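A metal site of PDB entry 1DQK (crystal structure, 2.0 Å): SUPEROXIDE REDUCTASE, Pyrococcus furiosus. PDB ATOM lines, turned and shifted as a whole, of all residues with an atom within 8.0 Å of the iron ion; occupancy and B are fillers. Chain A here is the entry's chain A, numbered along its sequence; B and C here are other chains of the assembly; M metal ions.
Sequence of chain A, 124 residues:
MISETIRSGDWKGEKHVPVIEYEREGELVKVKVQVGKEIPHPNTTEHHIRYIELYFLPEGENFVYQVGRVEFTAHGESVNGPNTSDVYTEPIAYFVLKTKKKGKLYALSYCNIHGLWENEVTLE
NE2 of His 16 binds the iron ion (2.0 Å).
ND1 of His 114 binds the iron ion.
The iron ion is bound by a ring nitrogen (NE2) of His 47 (2.1 Å).
The iron ion is bound by a ring nitrogen (NE2) of His 41, 2.3 Å away.
The iron ion is bound by the side-chain sulfur (SG) of Cys 111, 2.4 Å away.
The iron ion has five donor atoms within binding distance.
The backbone carbonyl oxygen (O) of His 114 lies within hydrogen-bond range of the indole nitrogen (NE1) of Trp 117 (3.0 Å).
N of Ile 113 sits close to SG of Cys 111 (3.6 Å).
The backbone NH (N) of His 16 is in hydrogen-bond range of the side-chain carboxylate (OE2) of Glu 14, at 3.0 Å.
The nearest printed residue that does not touch the iron ion is Ile 113 (4.5 Å).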
ATOM      1  N   GLU A  14      -1.116 -10.081  13.237  1.00  0.00           N
ATOM      2  CA  GLU A  14      -0.242  -9.627  14.317  1.00  0.00           C
ATOM      3  C   GLU A  14      -0.943  -8.765  15.368  1.00  0.00           C
ATOM      4  O   GLU A  14      -1.313  -7.622  15.104  1.00  0.00           O
ATOM      5  CB  GLU A  14       0.950  -8.868  13.723  1.00  0.00           C
ATOM      6  CG  GLU A  14       1.987  -8.470  14.758  1.00  0.00           C
ATOM      7  CD  GLU A  14       2.312  -9.606  15.724  1.00  0.00           C
ATOM      8  OE1 GLU A  14       2.865 -10.626  15.264  1.00  0.00           O
ATOM      9  OE2 GLU A  14       2.006  -9.470  16.931  1.00  0.00           O
ATOM     10  N   LYS A  15      -1.107  -9.319  16.569  1.00  0.00           N
ATOM     11  CA  LYS A  15      -1.777  -8.612  17.660  1.00  0.00           C
ATOM     12  C   LYS A  15      -1.051  -7.384  18.215  1.00  0.00           C
ATOM     13  O   LYS A  15      -1.683  -6.530  18.836  1.00  0.00           O
ATOM     14  CB  LYS A  15      -2.061  -9.596  18.801  1.00  0.00           C
ATOM     15  CG  LYS A  15      -0.825 -10.070  19.558  1.00  0.00           C
ATOM     16  CD  LYS A  15      -1.221 -10.923  20.762  1.00  0.00           C
ATOM     17  CE  LYS A  15      -1.479 -12.367  20.357  1.00  0.00           C
ATOM     18  NZ  LYS A  15      -0.221 -13.173  20.416  1.00  0.00           N
ATOM     19  N   HIS A  16       0.255  -7.292  18.014  1.00  0.00           N
ATOM     20  CA  HIS A  16       1.014  -6.162  18.535  1.00  0.00           C
ATOM     21  C   HIS A  16       0.919  -4.886  17.692  1.00  0.00           C
ATOM     22  O   HIS A  16       1.192  -3.789  18.197  1.00  0.00           O
ATOM     23  CB  HIS A  16       2.495  -6.533  18.662  1.00  0.00           C
ATOM     24  CG  HIS A  16       2.799  -7.372  19.861  1.00  0.00           C
ATOM     25  ND1 HIS A  16       2.928  -8.739  19.828  1.00  0.00           N
ATOM     26  CD2 HIS A  16       3.010  -7.016  21.150  1.00  0.00           C
ATOM     27  CE1 HIS A  16       3.211  -9.164  21.065  1.00  0.00           C
ATOM     28  NE2 HIS A  16       3.267  -8.153  21.903  1.00  0.00           N
ATOM     29  N   VAL A  35      -4.113  -1.372  20.374  1.00  0.00           N
ATOM     30  CA  VAL A  35      -3.351  -2.579  20.141  1.00  0.00           C
ATOM     31  C   VAL A  35      -4.246  -3.760  20.515  1.00  0.00           C
ATOM     32  O   VAL A  35      -4.766  -3.819  21.626  1.00  0.00           O
ATOM     33  CB  VAL A  35      -2.087  -2.611  21.027  1.00  0.00           C
ATOM     34  CG1 VAL A  35      -1.439  -3.983  20.963  1.00  0.00           C
ATOM     35  CG2 VAL A  35      -1.118  -1.516  20.568  1.00  0.00           C
ATOM     36  N   HIS A  41      -4.613  -8.382  22.999  1.00  0.00           N
ATOM     37  CA  HIS A  41      -3.278  -8.534  23.563  1.00  0.00           C
ATOM     38  C   HIS A  41      -3.386  -8.745  25.065  1.00  0.00           C
ATOM     39  O   HIS A  41      -4.242  -8.164  25.721  1.00  0.00           O
ATOM     40  CB  HIS A  41      -2.389  -7.316  23.280  1.00  0.00           C
ATOM     41  CG  HIS A  41      -0.967  -7.501  23.710  1.00  0.00           C
ATOM     42  ND1 HIS A  41      -0.525  -7.332  25.005  1.00  0.00           N
ATOM     43  CD2 HIS A  41       0.130  -7.865  22.992  1.00  0.00           C
ATOM     44  CE1 HIS A  41       0.794  -7.595  25.025  1.00  0.00           C
ATOM     45  NE2 HIS A  41       1.232  -7.920  23.828  1.00  0.00           N
ATOM     46  N   PRO A  42      -2.542  -9.620  25.625  1.00  0.00           N
ATOM     47  CA  PRO A  42      -2.628  -9.822  27.068  1.00  0.00           C
ATOM     48  C   PRO A  42      -2.404  -8.533  27.848  1.00  0.00           C
ATOM     49  O   PRO A  42      -1.746  -7.601  27.369  1.00  0.00           O
ATOM     50  CB  PRO A  42      -1.530 -10.846  27.342  1.00  0.00           C
ATOM     51  CG  PRO A  42      -1.321 -11.545  26.021  1.00  0.00           C
ATOM     52  CD  PRO A  42      -1.530 -10.479  24.994  1.00  0.00           C
ATOM     53  N   GLU A  46       2.791  -9.321  34.230  1.00  0.00           N
ATOM     54  CA  GLU A  46       3.985  -9.800  33.540  1.00  0.00           C
ATOM     55  C   GLU A  46       4.095  -9.472  32.062  1.00  0.00           C
ATOM     56  O   GLU A  46       5.199  -9.440  31.506  1.00  0.00           O
ATOM     57  CB  GLU A  46       4.091 -11.327  33.689  1.00  0.00           C
ATOM     58  CG  GLU A  46       4.100 -11.823  35.124  1.00  0.00           C
ATOM     59  CD  GLU A  46       2.702 -12.011  35.698  1.00  0.00           C
ATOM     60  OE1 GLU A  46       2.594 -12.350  36.894  1.00  0.00           O
ATOM     61  OE2 GLU A  46       1.717 -11.817  34.939  1.00  0.00           O
ATOM     62  N   HIS A  47       2.954  -9.220  31.416  1.00  0.00           N
ATOM     63  CA  HIS A  47       2.941  -8.961  29.966  1.00  0.00           C
ATOM     64  C   HIS A  47       1.832  -7.961  29.616  1.00  0.00           C
ATOM     65  O   HIS A  47       0.646  -8.237  29.799  1.00  0.00           O
ATOM     66  CB  HIS A  47       2.701 -10.306  29.267  1.00  0.00           C
ATOM     67  CG  HIS A  47       2.757 -10.247  27.771  1.00  0.00           C
ATOM     68  ND1 HIS A  47       2.275 -11.236  26.944  1.00  0.00           N
ATOM     69  CD2 HIS A  47       3.212  -9.273  26.941  1.00  0.00           C
ATOM     70  CE1 HIS A  47       2.448 -10.847  25.677  1.00  0.00           C
ATOM     71  NE2 HIS A  47       3.012  -9.653  25.628  1.00  0.00           N
ATOM     72  N   HIS A  48       2.228  -6.799  29.089  1.00  0.00           N
ATOM     73  CA  HIS A  48       1.234  -5.761  28.767  1.00  0.00           C
ATOM     74  C   HIS A  48       1.796  -4.653  27.879  1.00  0.00           C
ATOM     75  O   HIS A  48       3.001  -4.457  27.805  1.00  0.00           O
ATOM     76  CB  HIS A  48       0.749  -5.124  30.064  1.00  0.00           C
ATOM     77  CG  HIS A  48       1.852  -4.560  30.889  1.00  0.00           C
ATOM     78  ND1 HIS A  48       2.366  -5.198  31.996  1.00  0.00           N
ATOM     79  CD2 HIS A  48       2.571  -3.419  30.758  1.00  0.00           C
ATOM     80  CE1 HIS A  48       3.347  -4.480  32.515  1.00  0.00           C
ATOM     81  NE2 HIS A  48       3.497  -3.393  31.781  1.00  0.00           N
ATOM     82  N   ILE A  49       0.904  -3.918  27.226  1.00  0.00           N
ATOM     83  CA  ILE A  49       1.321  -2.796  26.375  1.00  0.00           C
ATOM     84  C   ILE A  49       1.487  -1.593  27.300  1.00  0.00           C
ATOM     85  O   ILE A  49       0.552  -1.235  28.018  1.00  0.00           O
ATOM     86  CB  ILE A  49       0.250  -2.468  25.307  1.00  0.00           C
ATOM     87  CG1 ILE A  49       0.004  -3.704  24.433  1.00  0.00           C
ATOM     88  CG2 ILE A  49       0.707  -1.274  24.449  1.00  0.00           C
ATOM     89  CD1 ILE A  49       1.259  -4.268  23.771  1.00  0.00           C
ATOM     90  N   TYR A 110       4.707   0.157  22.550  1.00  0.00           N
ATOM     91  CA  TYR A 110       5.723  -0.640  23.232  1.00  0.00           C
ATOM     92  C   TYR A 110       5.130  -1.687  24.184  1.00  0.00           C
ATOM     93  O   TYR A 110       4.333  -1.354  25.082  1.00  0.00           O
ATOM     94  CB  TYR A 110       6.672   0.287  24.007  1.00  0.00           C
ATOM     95  CG  TYR A 110       7.732  -0.422  24.832  1.00  0.00           C
ATOM     96  CD1 TYR A 110       8.834  -1.022  24.213  1.00  0.00           C
ATOM     97  CD2 TYR A 110       7.631  -0.501  26.226  1.00  0.00           C
ATOM     98  CE1 TYR A 110       9.824  -1.686  24.959  1.00  0.00           C
ATOM     99  CE2 TYR A 110       8.605  -1.173  26.988  1.00  0.00           C
ATOM    100  CZ  TYR A 110       9.695  -1.758  26.340  1.00  0.00           C
ATOM    101  OH  TYR A 110      10.644  -2.434  27.082  1.00  0.00           O
ATOM    102  N   CYS A 111       5.503  -2.940  23.966  1.00  0.00           N
ATOM    103  CA  CYS A 111       5.063  -4.043  24.815  1.00  0.00           C
ATOM    104  C   CYS A 111       6.225  -4.221  25.805  1.00  0.00           C
ATOM    105  O   CYS A 111       7.379  -4.107  25.409  1.00  0.00           O
ATOM    106  CB  CYS A 111       4.875  -5.329  23.995  1.00  0.00           C
ATOM    107  SG  CYS A 111       4.559  -6.806  25.003  1.00  0.00           S
ATOM    108  N   ASN A 112       5.925  -4.501  27.067  1.00  0.00           N
ATOM    109  CA  ASN A 112       6.988  -4.651  28.057  1.00  0.00           C
ATOM    110  C   ASN A 112       7.937  -5.827  27.806  1.00  0.00           C
ATOM    111  O   ASN A 112       9.028  -5.853  28.359  1.00  0.00           O
ATOM    112  CB  ASN A 112       6.392  -4.715  29.478  1.00  0.00           C
ATOM    113  CG  ASN A 112       5.721  -6.036  29.780  1.00  0.00           C
ATOM    114  OD1 ASN A 112       5.249  -6.732  28.884  1.00  0.00           O
ATOM    115  ND2 ASN A 112       5.670  -6.390  31.057  1.00  0.00           N
ATOM    116  N   ILE A 113       7.551  -6.778  26.945  1.00  0.00           N
ATOM    117  CA  ILE A 113       8.456  -7.891  26.655  1.00  0.00           C
ATOM    118  C   ILE A 113       8.667  -8.172  25.172  1.00  0.00           C
ATOM    119  O   ILE A 113       9.567  -8.933  24.807  1.00  0.00           O
ATOM    120  CB  ILE A 113       7.995  -9.244  27.310  1.00  0.00           C
ATOM    121  CG1 ILE A 113       6.652  -9.689  26.717  1.00  0.00           C
ATOM    122  CG2 ILE A 113       7.914  -9.107  28.826  1.00  0.00           C
ATOM    123  CD1 ILE A 113       6.132 -10.982  27.316  1.00  0.00           C
ATOM    124  N   HIS A 114       7.865  -7.555  24.314  1.00  0.00           N
ATOM    125  CA  HIS A 114       7.971  -7.781  22.868  1.00  0.00           C
ATOM    126  C   HIS A 114       8.491  -6.586  22.068  1.00  0.00           C
ATOM    127  O   HIS A 114       8.323  -6.522  20.842  1.00  0.00           O
ATOM    128  CB  HIS A 114       6.608  -8.198  22.316  1.00  0.00           C
ATOM    129  CG  HIS A 114       6.195  -9.592  22.692  1.00  0.00           C
ATOM    130  ND1 HIS A 114       4.999  -9.847  23.316  1.00  0.00           N
ATOM    131  CD2 HIS A 114       6.845 -10.760  22.461  1.00  0.00           C
ATOM    132  CE1 HIS A 114       4.941 -11.166  23.449  1.00  0.00           C
ATOM    133  NE2 HIS A 114       6.031 -11.756  22.944  1.00  0.00           N
ATOM    134  N   GLY A 115       9.131  -5.652  22.750  1.00  0.00           N
ATOM    135  CA  GLY A 115       9.706  -4.505  22.068  1.00  0.00           C
ATOM    136  C   GLY A 115       8.771  -3.479  21.455  1.00  0.00           C
ATOM    137  O   GLY A 115       7.585  -3.399  21.805  1.00  0.00           O
ATOM    138  N   TRP A 117       6.699  -1.414  18.354  1.00  0.00           N
ATOM    139  CA  TRP A 117       5.845  -1.716  17.212  1.00  0.00           C
ATOM    140  C   TRP A 117       5.328  -0.432  16.569  1.00  0.00           C
ATOM    141  O   TRP A 117       5.084   0.567  17.266  1.00  0.00           O
ATOM    142  CB  TRP A 117       4.680  -2.595  17.653  1.00  0.00           C
ATOM    143  CG  TRP A 117       5.101  -3.964  18.064  1.00  0.00           C
ATOM    144  CD1 TRP A 117       5.611  -4.326  19.284  1.00  0.00           C
ATOM    145  CD2 TRP A 117       5.086  -5.149  17.274  1.00  0.00           C
ATOM    146  NE1 TRP A 117       5.909  -5.664  19.281  1.00  0.00           N
ATOM    147  CE2 TRP A 117       5.601  -6.202  18.061  1.00  0.00           C
ATOM    148  CE3 TRP A 117       4.683  -5.432  15.961  1.00  0.00           C
ATOM    149  CZ2 TRP A 117       5.723  -7.508  17.588  1.00  0.00           C
ATOM    150  CZ3 TRP A 117       4.805  -6.738  15.487  1.00  0.00           C
ATOM    151  CH2 TRP A 117       5.327  -7.765  16.305  1.00  0.00           C
ATOM    152  N   VAL B  79      10.012 -12.580  27.795  1.00  0.00           N
ATOM    153  CA  VAL B  79       9.157 -13.644  27.257  1.00  0.00           C
ATOM    154  C   VAL B  79       9.326 -14.933  28.078  1.00  0.00           C
ATOM    155  O   VAL B  79       8.559 -15.893  27.928  1.00  0.00           O
ATOM    156  CB  VAL B  79       9.542 -13.976  25.810  1.00  0.00           C
ATOM    157  CG1 VAL B  79       9.018 -12.900  24.873  1.00  0.00           C
ATOM    158  CG2 VAL B  79      11.065 -14.094  25.712  1.00  0.00           C
ATOM    159  N   PHE C  63      14.091  -8.815  21.199  1.00  0.00           N
ATOM    160  CA  PHE C  63      13.243  -7.716  21.625  1.00  0.00           C
ATOM    161  C   PHE C  63      13.987  -6.656  22.425  1.00  0.00           C
ATOM    162  O   PHE C  63      14.698  -6.961  23.387  1.00  0.00           O
ATOM    163  CB  PHE C  63      12.049  -8.279  22.402  1.00  0.00           C
ATOM    164  CG  PHE C  63      11.281  -9.323  21.633  1.00  0.00           C
ATOM    165  CD1 PHE C  63      11.442 -10.673  21.904  1.00  0.00           C
ATOM    166  CD2 PHE C  63      10.419  -8.954  20.598  1.00  0.00           C
ATOM    167  CE1 PHE C  63      10.769 -11.652  21.151  1.00  0.00           C
ATOM    168  CE2 PHE C  63       9.733  -9.912  19.847  1.00  0.00           C
ATOM    169  CZ  PHE C  63       9.917 -11.262  20.116  1.00  0.00           C
HETATM  170 FE    FE M   1       3.421  -8.598  23.814  1.00  0.00          FE
